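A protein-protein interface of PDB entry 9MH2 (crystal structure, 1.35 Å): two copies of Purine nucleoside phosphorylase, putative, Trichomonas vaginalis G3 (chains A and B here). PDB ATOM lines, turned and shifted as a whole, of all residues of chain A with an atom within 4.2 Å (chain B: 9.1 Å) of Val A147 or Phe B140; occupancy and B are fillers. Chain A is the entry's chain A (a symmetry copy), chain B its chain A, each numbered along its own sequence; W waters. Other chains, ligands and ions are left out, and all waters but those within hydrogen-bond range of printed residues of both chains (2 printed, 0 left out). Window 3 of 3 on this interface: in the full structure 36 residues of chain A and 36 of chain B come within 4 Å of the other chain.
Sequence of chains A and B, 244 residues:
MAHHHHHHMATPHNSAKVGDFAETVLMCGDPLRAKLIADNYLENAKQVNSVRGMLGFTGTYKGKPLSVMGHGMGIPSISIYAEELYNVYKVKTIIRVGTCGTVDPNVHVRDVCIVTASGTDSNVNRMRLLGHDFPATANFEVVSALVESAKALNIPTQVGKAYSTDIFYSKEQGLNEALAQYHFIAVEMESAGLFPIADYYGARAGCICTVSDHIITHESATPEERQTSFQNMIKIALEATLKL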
ATOM      1  N   ILE A 114      10.807  13.506  23.701  1.00  0.00           N
ATOM      2  CA  ILE A 114       9.519  13.112  24.253  1.00  0.00           C
ATOM      3  C   ILE A 114       8.441  13.654  23.321  1.00  0.00           C
ATOM      4  O   ILE A 114       8.384  14.863  23.059  1.00  0.00           O
ATOM      5  CB  ILE A 114       9.349  13.640  25.684  1.00  0.00           C
ATOM      6  CG1 ILE A 114      10.354  12.935  26.617  1.00  0.00           C
ATOM      7  CG2 ILE A 114       7.942  13.389  26.159  1.00  0.00           C
ATOM      8  CD1 ILE A 114      10.492  13.595  27.995  1.00  0.00           C
ATOM      9  N   PHE A 140      -1.500  13.479  28.115  1.00  0.00           N
ATOM     10  CA  PHE A 140      -0.726  14.496  28.811  1.00  0.00           C
ATOM     11  C   PHE A 140      -0.069  13.955  30.085  1.00  0.00           C
ATOM     12  O   PHE A 140       1.059  14.333  30.407  1.00  0.00           O
ATOM     13  CB  PHE A 140      -1.586  15.714  29.119  1.00  0.00           C
ATOM     14  CG  PHE A 140      -0.868  16.739  29.950  1.00  0.00           C
ATOM     15  CD1 PHE A 140       0.052  17.596  29.368  1.00  0.00           C
ATOM     16  CD2 PHE A 140      -1.056  16.794  31.326  1.00  0.00           C
ATOM     17  CE1 PHE A 140       0.733  18.540  30.133  1.00  0.00           C
ATOM     18  CE2 PHE A 140      -0.380  17.733  32.102  1.00  0.00           C
ATOM     19  CZ  PHE A 140       0.525  18.601  31.498  1.00  0.00           C
ATOM     20  N   VAL A 143       3.080  12.190  28.955  1.00  0.00           N
ATOM     21  CA  VAL A 143       4.127  13.134  28.577  1.00  0.00           C
ATOM     22  C   VAL A 143       4.743  13.753  29.825  1.00  0.00           C
ATOM     23  O   VAL A 143       5.967  13.853  29.958  1.00  0.00           O
ATOM     24  CB  VAL A 143       3.569  14.220  27.639  1.00  0.00           C
ATOM     25  CG1 VAL A 143       4.659  15.252  27.328  1.00  0.00           C
ATOM     26  CG2 VAL A 143       3.016  13.628  26.350  1.00  0.00           C
ATOM     27  N   SER A 144       3.890  14.197  30.749  1.00  0.00           N
ATOM     28  CA  SER A 144       4.378  14.856  31.959  1.00  0.00           C
ATOM     29  C   SER A 144       5.212  13.909  32.805  1.00  0.00           C
ATOM     30  O   SER A 144       6.232  14.312  33.373  1.00  0.00           O
ATOM     31  CB  SER A 144       3.200  15.375  32.780  1.00  0.00           C
ATOM     32  OG  SER A 144       3.654  15.960  33.993  1.00  0.00           O
ATOM     33  N   ALA A 145       4.782  12.656  32.922  1.00  0.00           N
ATOM     34  CA  ALA A 145       5.558  11.690  33.692  1.00  0.00           C
ATOM     35  C   ALA A 145       6.947  11.507  33.094  1.00  0.00           C
ATOM     36  O   ALA A 145       7.934  11.428  33.825  1.00  0.00           O
ATOM     37  CB  ALA A 145       4.819  10.361  33.784  1.00  0.00           C
ATOM     38  N   LEU A 146       7.047  11.457  31.761  1.00  0.00           N
ATOM     39  CA  LEU A 146       8.349  11.345  31.114  1.00  0.00           C
ATOM     40  C   LEU A 146       9.192  12.593  31.338  1.00  0.00           C
ATOM     41  O   LEU A 146      10.381  12.501  31.662  1.00  0.00           O
ATOM     42  CB  LEU A 146       8.146  11.092  29.620  1.00  0.00           C
ATOM     43  CG  LEU A 146       7.573   9.718  29.272  1.00  0.00           C
ATOM     44  CD1 LEU A 146       7.068   9.723  27.823  1.00  0.00           C
ATOM     45  CD2 LEU A 146       8.589   8.588  29.434  1.00  0.00           C
ATOM     46  N   VAL A 147       8.592  13.773  31.193  1.00  0.00           N
ATOM     47  CA  VAL A 147       9.332  15.017  31.379  1.00  0.00           C
ATOM     48  C   VAL A 147       9.848  15.114  32.809  1.00  0.00           C
ATOM     49  O   VAL A 147      11.004  15.476  33.047  1.00  0.00           O
ATOM     50  CB  VAL A 147       8.450  16.223  31.008  1.00  0.00           C
ATOM     51  CG1 VAL A 147       9.089  17.529  31.489  1.00  0.00           C
ATOM     52  CG2 VAL A 147       8.191  16.278  29.511  1.00  0.00           C
ATOM     53  N   GLU A 148       8.984  14.822  33.781  1.00  0.00           N
ATOM     54  CA  GLU A 148       9.372  14.936  35.183  1.00  0.00           C
ATOM     55  C   GLU A 148      10.414  13.895  35.558  1.00  0.00           C
ATOM     56  O   GLU A 148      11.326  14.181  36.335  1.00  0.00           O
ATOM     57  CB  GLU A 148       8.135  14.793  36.059  1.00  0.00           C
ATOM     58  CG  GLU A 148       7.187  15.944  35.923  1.00  0.00           C
ATOM     59  CD  GLU A 148       7.855  17.293  36.182  1.00  0.00           C
ATOM     60  OE1 GLU A 148       8.450  17.468  37.274  1.00  0.00           O
ATOM     61  OE2 GLU A 148       7.805  18.169  35.284  1.00  0.00           O
ATOM     62  N   SER A 149      10.316  12.691  34.997  1.00  0.00           N
ATOM     63  CA  SER A 149      11.317  11.672  35.289  1.00  0.00           C
ATOM     64  C   SER A 149      12.684  12.090  34.769  1.00  0.00           C
ATOM     65  O   SER A 149      13.690  11.938  35.471  1.00  0.00           O
ATOM     66  CB  SER A 149      10.901  10.328  34.696  1.00  0.00           C
ATOM     67  OG  SER A 149       9.717   9.844  35.304  1.00  0.00           O
ATOM     68  N   ALA A 150      12.738  12.640  33.550  1.00  0.00           N
ATOM     69  CA  ALA A 150      14.017  13.093  33.007  1.00  0.00           C
ATOM     70  C   ALA A 150      14.600  14.220  33.849  1.00  0.00           C
ATOM     71  O   ALA A 150      15.810  14.257  34.098  1.00  0.00           O
ATOM     72  CB  ALA A 150      13.843  13.530  31.553  1.00  0.00           C
ATOM     73  N   LYS A 151      13.755  15.146  34.304  1.00  0.00           N
ATOM     74  CA  LYS A 151      14.232  16.225  35.169  1.00  0.00           C
ATOM     75  C   LYS A 151      14.854  15.677  36.448  1.00  0.00           C
ATOM     76  O   LYS A 151      15.922  16.130  36.872  1.00  0.00           O
ATOM     77  CB  LYS A 151      13.080  17.168  35.514  1.00  0.00           C
ATOM     78  CG  LYS A 151      12.644  18.056  34.370  1.00  0.00           C
ATOM     79  CD  LYS A 151      11.288  18.717  34.641  1.00  0.00           C
ATOM     80  CE  LYS A 151      11.383  19.903  35.585  1.00  0.00           C
ATOM     81  NZ  LYS A 151      10.570  21.046  35.048  1.00  0.00           N
ATOM     82  N   VAL A 159      11.094  18.182  23.636  1.00  0.00           N
ATOM     83  CA  VAL A 159       9.680  17.832  23.750  1.00  0.00           C
ATOM     84  C   VAL A 159       8.966  18.429  22.544  1.00  0.00           C
ATOM     85  O   VAL A 159       9.037  19.642  22.321  1.00  0.00           O
ATOM     86  CB  VAL A 159       9.082  18.390  25.058  1.00  0.00           C
ATOM     87  CG1 VAL A 159       7.627  17.995  25.204  1.00  0.00           C
ATOM     88  CG2 VAL A 159       9.885  17.902  26.265  1.00  0.00           C
ATOM     89  N   ILE B 114      -8.266  22.179  28.547  1.00  0.00           N
ATOM     90  CA  ILE B 114      -6.940  22.592  28.111  1.00  0.00           C
ATOM     91  C   ILE B 114      -6.555  21.708  26.931  1.00  0.00           C
ATOM     92  O   ILE B 114      -6.547  20.475  27.044  1.00  0.00           O
ATOM     93  CB  ILE B 114      -5.925  22.483  29.257  1.00  0.00           C
ATOM     94  CG1 ILE B 114      -6.266  23.517  30.349  1.00  0.00           C
ATOM     95  CG2 ILE B 114      -4.534  22.726  28.733  1.00  0.00           C
ATOM     96  CD1 ILE B 114      -5.519  23.295  31.670  1.00  0.00           C
ATOM     97  N   VAL B 115      -6.237  22.333  25.804  1.00  0.00           N
ATOM     98  CA  VAL B 115      -6.099  21.639  24.530  1.00  0.00           C
ATOM     99  C   VAL B 115      -4.649  21.225  24.305  1.00  0.00           C
ATOM    100  O   VAL B 115      -3.747  22.067  24.277  1.00  0.00           O
ATOM    101  CB  VAL B 115      -6.594  22.541  23.393  1.00  0.00           C
ATOM    102  CG1 VAL B 115      -6.387  21.878  22.056  1.00  0.00           C
ATOM    103  CG2 VAL B 115      -8.056  22.878  23.609  1.00  0.00           C
ATOM    104  N   THR B 116      -4.428  19.931  24.076  1.00  0.00           N
ATOM    105  CA  THR B 116      -3.089  19.455  23.748  1.00  0.00           C
ATOM    106  C   THR B 116      -2.828  19.429  22.243  1.00  0.00           C
ATOM    107  O   THR B 116      -1.688  19.614  21.813  1.00  0.00           O
ATOM    108  CB  THR B 116      -2.893  18.043  24.297  1.00  0.00           C
ATOM    109  OG1 THR B 116      -3.996  17.233  23.885  1.00  0.00           O
ATOM    110  CG2 THR B 116      -2.790  18.064  25.823  1.00  0.00           C
ATOM    111  N   THR B 137      -0.472  21.049  17.249  1.00  0.00           N
ATOM    112  CA  THR B 137      -0.066  20.619  18.582  1.00  0.00           C
ATOM    113  C   THR B 137       0.308  21.829  19.430  1.00  0.00           C
ATOM    114  O   THR B 137       1.108  22.671  19.011  1.00  0.00           O
ATOM    115  CB  THR B 137       1.118  19.644  18.464  1.00  0.00           C
ATOM    116  OG1 THR B 137       0.801  18.635  17.496  1.00  0.00           O
ATOM    117  CG2 THR B 137       1.421  18.988  19.799  1.00  0.00           C
ATOM    118  N   ALA B 138      -0.259  21.899  20.624  1.00  0.00           N
ATOM    119  CA  ALA B 138       0.084  22.967  21.550  1.00  0.00           C
ATOM    120  C   ALA B 138       1.491  22.757  22.099  1.00  0.00           C
ATOM    121  O   ALA B 138       1.988  21.628  22.204  1.00  0.00           O
ATOM    122  CB  ALA B 138      -0.908  23.004  22.710  1.00  0.00           C
ATOM    123  N   ASN B 139       2.142  23.864  22.428  1.00  0.00           N
ATOM    124  CA  ASN B 139       3.457  23.799  23.043  1.00  0.00           C
ATOM    125  C   ASN B 139       3.352  23.236  24.459  1.00  0.00           C
ATOM    126  O   ASN B 139       2.474  23.619  25.240  1.00  0.00           O
ATOM    127  CB  ASN B 139       4.067  25.195  23.085  1.00  0.00           C
ATOM    128  CG  ASN B 139       5.318  25.258  23.937  1.00  0.00           C
ATOM    129  OD1 ASN B 139       5.264  25.561  25.138  1.00  0.00           O
ATOM    130  ND2 ASN B 139       6.455  24.985  23.323  1.00  0.00           N
ATOM    131  N   PHE B 140       4.257  22.314  24.792  1.00  0.00           N
ATOM    132  CA  PHE B 140       4.127  21.616  26.063  1.00  0.00           C
ATOM    133  C   PHE B 140       4.281  22.558  27.261  1.00  0.00           C
ATOM    134  O   PHE B 140       3.589  22.397  28.268  1.00  0.00           O
ATOM    135  CB  PHE B 140       5.117  20.462  26.149  1.00  0.00           C
ATOM    136  CG  PHE B 140       5.113  19.790  27.493  1.00  0.00           C
ATOM    137  CD1 PHE B 140       4.111  18.893  27.827  1.00  0.00           C
ATOM    138  CD2 PHE B 140       6.066  20.115  28.451  1.00  0.00           C
ATOM    139  CE1 PHE B 140       4.091  18.276  29.075  1.00  0.00           C
ATOM    140  CE2 PHE B 140       6.055  19.505  29.704  1.00  0.00           C
ATOM    141  CZ  PHE B 140       5.054  18.590  30.015  1.00  0.00           C
ATOM    142  N   GLU B 141       5.195  23.530  27.184  1.00  0.00           N
ATOM    143  CA  GLU B 141       5.359  24.470  28.290  1.00  0.00           C
ATOM    144  C   GLU B 141       4.080  25.275  28.509  1.00  0.00           C
ATOM    145  O   GLU B 141       3.708  25.567  29.652  1.00  0.00           O
ATOM    146  CB  GLU B 141       6.558  25.385  28.025  1.00  0.00           C
ATOM    147  CG  GLU B 141       7.915  24.675  27.893  1.00  0.00           C
ATOM    148  CD  GLU B 141       8.143  24.067  26.483  1.00  0.00           C
ATOM    149  OE1 GLU B 141       7.655  22.945  26.198  1.00  0.00           O
ATOM    150  OE2 GLU B 141       8.812  24.715  25.641  1.00  0.00           O
ATOM    151  N   VAL B 142       3.372  25.614  27.432  1.00  0.00           N
ATOM    152  CA  VAL B 142       2.112  26.339  27.569  1.00  0.00           C
ATOM    153  C   VAL B 142       1.043  25.450  28.198  1.00  0.00           C
ATOM    154  O   VAL B 142       0.333  25.862  29.119  1.00  0.00           O
ATOM    155  CB  VAL B 142       1.656  26.912  26.216  1.00  0.00           C
ATOM    156  CG1 VAL B 142       0.293  27.547  26.369  1.00  0.00           C
ATOM    157  CG2 VAL B 142       2.654  27.937  25.715  1.00  0.00           C
ATOM    158  N   VAL B 143       0.911  24.214  27.714  1.00  0.00           N
ATOM    159  CA  VAL B 143      -0.068  23.304  28.301  1.00  0.00           C
ATOM    160  C   VAL B 143       0.213  23.129  29.787  1.00  0.00           C
ATOM    161  O   VAL B 143      -0.692  23.187  30.625  1.00  0.00           O
ATOM    162  CB  VAL B 143      -0.056  21.947  27.573  1.00  0.00           C
ATOM    163  CG1 VAL B 143      -1.022  20.976  28.261  1.00  0.00           C
ATOM    164  CG2 VAL B 143      -0.409  22.091  26.099  1.00  0.00           C
ATOM    165  N   SER B 144       1.480  22.890  30.127  1.00  0.00           N
ATOM    166  CA  SER B 144       1.847  22.654  31.522  1.00  0.00           C
ATOM    167  C   SER B 144       1.571  23.878  32.380  1.00  0.00           C
ATOM    168  O   SER B 144       1.111  23.753  33.519  1.00  0.00           O
ATOM    169  CB  SER B 144       3.325  22.284  31.617  1.00  0.00           C
ATOM    170  OG  SER B 144       3.714  22.117  32.974  1.00  0.00           O
ATOM    171  N   ALA B 145       1.869  25.066  31.861  1.00  0.00           N
ATOM    172  CA  ALA B 145       1.595  26.280  32.621  1.00  0.00           C
ATOM    173  C   ALA B 145       0.107  26.415  32.915  1.00  0.00           C
ATOM    174  O   ALA B 145      -0.277  26.792  34.023  1.00  0.00           O
ATOM    175  CB  ALA B 145       2.123  27.504  31.883  1.00  0.00           C
ATOM    176  N   LEU B 146      -0.750  26.090  31.941  1.00  0.00           N
ATOM    177  CA  LEU B 146      -2.190  26.133  32.168  1.00  0.00           C
ATOM    178  C   LEU B 146      -2.626  25.086  33.184  1.00  0.00           C
ATOM    179  O   LEU B 146      -3.410  25.379  34.093  1.00  0.00           O
ATOM    180  CB  LEU B 146      -2.913  25.928  30.837  1.00  0.00           C
ATOM    181  CG  LEU B 146      -2.779  27.084  29.846  1.00  0.00           C
ATOM    182  CD1 LEU B 146      -3.207  26.617  28.448  1.00  0.00           C
ATOM    183  CD2 LEU B 146      -3.615  28.303  30.234  1.00  0.00           C
ATOM    184  N   VAL B 147      -2.113  23.863  33.064  1.00  0.00           N
ATOM    185  CA  VAL B 147      -2.488  22.800  33.991  1.00  0.00           C
ATOM    186  C   VAL B 147      -2.070  23.165  35.409  1.00  0.00           C
ATOM    187  O   VAL B 147      -2.835  22.997  36.363  1.00  0.00           O
ATOM    188  CB  VAL B 147      -1.874  21.461  33.543  1.00  0.00           C
ATOM    189  CG1 VAL B 147      -1.992  20.414  34.654  1.00  0.00           C
ATOM    190  CG2 VAL B 147      -2.526  20.956  32.265  1.00  0.00           C
ATOM    191  N   GLU B 148      -0.835  23.642  35.568  1.00  0.00           N
ATOM    192  CA  GLU B 148      -0.327  23.971  36.896  1.00  0.00           C
ATOM    193  C   GLU B 148      -1.053  25.169  37.487  1.00  0.00           C
ATOM    194  O   GLU B 148      -1.316  25.205  38.690  1.00  0.00           O
ATOM    195  CB  GLU B 148       1.168  24.242  36.809  1.00  0.00           C
ATOM    196  CG  GLU B 148       1.966  23.016  36.487  1.00  0.00           C
ATOM    197  CD  GLU B 148       1.700  21.868  37.457  1.00  0.00           C
ATOM    198  OE1 GLU B 148       1.867  22.070  38.685  1.00  0.00           O
ATOM    199  OE2 GLU B 148       1.304  20.770  36.993  1.00  0.00           O
ATOM    200  N   VAL B 159      -8.097  17.730  30.003  1.00  0.00           N
ATOM    201  CA  VAL B 159      -6.918  17.963  29.172  1.00  0.00           C
ATOM    202  C   VAL B 159      -6.981  16.982  28.009  1.00  0.00           C
ATOM    203  O   VAL B 159      -7.053  15.767  28.227  1.00  0.00           O
ATOM    204  CB  VAL B 159      -5.625  17.750  29.985  1.00  0.00           C
ATOM    205  CG1 VAL B 159      -4.398  18.031  29.142  1.00  0.00           C
ATOM    206  CG2 VAL B 159      -5.623  18.636  31.232  1.00  0.00           C
ATOM    207  N   ASP B 199       4.451  27.144  15.183  1.00  0.00           N
ATOM    208  CA  ASP B 199       5.574  26.296  14.784  1.00  0.00           C
ATOM    209  C   ASP B 199       6.434  26.985  13.731  1.00  0.00           C
ATOM    210  O   ASP B 199       7.666  26.987  13.823  1.00  0.00           O
ATOM    211  CB  ASP B 199       5.088  24.963  14.218  1.00  0.00           C
ATOM    212  CG  ASP B 199       4.509  24.042  15.254  1.00  0.00           C
ATOM    213  OD1 ASP B 199       4.830  24.191  16.452  1.00  0.00           O
ATOM    214  OD2 ASP B 199       3.749  23.126  14.847  1.00  0.00           O
ATOM    215  N   ALA B 203       7.792  29.717  17.693  1.00  0.00           N
ATOM    216  CA  ALA B 203       7.137  30.361  18.820  1.00  0.00           C
ATOM    217  C   ALA B 203       6.195  29.358  19.483  1.00  0.00           C
ATOM    218  O   ALA B 203       6.173  28.174  19.147  1.00  0.00           O
ATOM    219  CB  ALA B 203       6.402  31.617  18.335  1.00  0.00           C
ATOM    220  N   ARG B 204       5.392  29.847  20.421  1.00  0.00           N
ATOM    221  CA  ARG B 204       4.607  28.996  21.298  1.00  0.00           C
ATOM    222  C   ARG B 204       3.138  29.386  21.258  1.00  0.00           C
ATOM    223  O   ARG B 204       2.793  30.569  21.168  1.00  0.00           O
ATOM    224  CB  ARG B 204       5.131  29.096  22.747  1.00  0.00           C
ATOM    225  CG  ARG B 204       6.513  28.505  22.903  1.00  0.00           C
ATOM    226  CD  ARG B 204       6.905  28.439  24.339  1.00  0.00           C
ATOM    227  NE  ARG B 204       6.786  29.732  24.983  1.00  0.00           N
ATOM    228  CZ  ARG B 204       7.193  29.979  26.216  1.00  0.00           C
ATOM    229  NH1 ARG B 204       7.795  29.043  26.943  1.00  0.00           N
ATOM    230  NH2 ARG B 204       7.008  31.194  26.727  1.00  0.00           N
ATOM    231  N   ALA B 205       2.274  28.380  21.373  1.00  0.00           N
ATOM    232  CA  ALA B 205       0.841  28.601  21.413  1.00  0.00           C
ATOM    233  C   ALA B 205       0.159  27.530  22.248  1.00  0.00           C
ATOM    234  O   ALA B 205       0.658  26.401  22.374  1.00  0.00           O
ATOM    235  CB  ALA B 205       0.214  28.651  20.019  1.00  0.00           C
ATOM    236  N   GLY B 206      -0.995  27.890  22.806  1.00  0.00           N
ATOM    237  CA  GLY B 206      -1.862  26.936  23.461  1.00  0.00           C
ATOM    238  C   GLY B 206      -3.289  27.437  23.410  1.00  0.00           C
ATOM    239  O   GLY B 206      -3.575  28.489  22.838  1.00  0.00           O
ATOM    240  N   LEU B 244       5.364  32.076  31.575  1.00  0.00           N
ATOM    241  CA  LEU B 244       5.665  31.936  30.147  1.00  0.00           C
ATOM    242  C   LEU B 244       6.318  33.193  29.560  1.00  0.00           C
ATOM    243  O   LEU B 244       6.766  33.205  28.408  1.00  0.00           O
ATOM    244  CB  LEU B 244       4.386  31.626  29.359  1.00  0.00           C
ATOM    245  CG  LEU B 244       3.679  30.304  29.673  1.00  0.00           C
ATOM    246  CD1 LEU B 244       2.278  30.308  29.089  1.00  0.00           C
ATOM    247  CD2 LEU B 244       4.479  29.105  29.160  1.00  0.00           C
ATOM    248  OXT LEU B 244       6.411  34.231  30.207  1.00  0.00           O
HETATM  249  O   HOH W   1       6.364  21.372  23.055  1.00  0.00           O
HETATM  250  O   HOH W   2      -4.300  14.078  27.737  1.00  0.00           O
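Printed residues of chain B within 4 Å of Phe A140: Phe B140, Val B143, Val B147 and Val B159. Of the printed residues of chain B, Val A143 touches Phe B140. Of chain B, only Phe B140 comes within 4 Å of Val A147. Printed residues of chain A within 4 Å of Phe B140: Phe A140 (3.5 Å), Val A143 (3.5 Å), Val A147 (3.9 Å) and Val A159 (3.6 Å). Of the printed residues of chain A, Val B143 touches Phe A140 (3.5 Å). Printed residues of chain A within 4 Å of Val B159: Phe A140. The nearest printed residue of chain B that does not touch Val A147 is Ser B144 (7.2 Å). The nearest printed residue of chain B that does not touch Val A143 is Thr B116 (7.3 Å).
Water W1 lies within hydrogen-bond range of the backbone NH (N) of Phe B140 and the backbone carbonyl oxygen (O) of Val A159. Water W2 lies within hydrogen-bond range of the backbone NH (N) of Phe A140 and the backbone carbonyl oxygen (O) of Val B159.
Of the 22 printed residues of chain B, 4 touch a printed residue of chain A. Of the 12 printed residues of chain A, 4 touch a printed residue of chain B. Hydrophobic or aromatic side chains of chain A within 4 Å of the printed part of chain B: Phe A140, Val A143, Val A147 and Val A159.
Phe B140 touches its own counterpart, Phe A140. Phe A140 touches Val B143, and with the chains exchanged Val A143 touches Phe B140. Phe A140 touches Val B147, and with the chains exchanged Val A147 touches Phe B140. Phe A140 touches Val B159, and with the chains exchanged Val A159 touches Phe B140. Positions printed for both chains: 114, 140, 143, 144, 145, 146, 147, 148 and 159. Of the 7 pairs that touch across the chains among the printed residues, 7 have their exchanged pair printed and touching as well.
Phe B140 touches Phe A140. Val B143 touches Phe A140. Val B147 touches Phe A140. CB of Phe A140 touches CG1 of Val B159, 3.6 Å away. Val A143 touches Phe B140. Phe B140 touches Val A147. Val A159 touches Phe B140.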
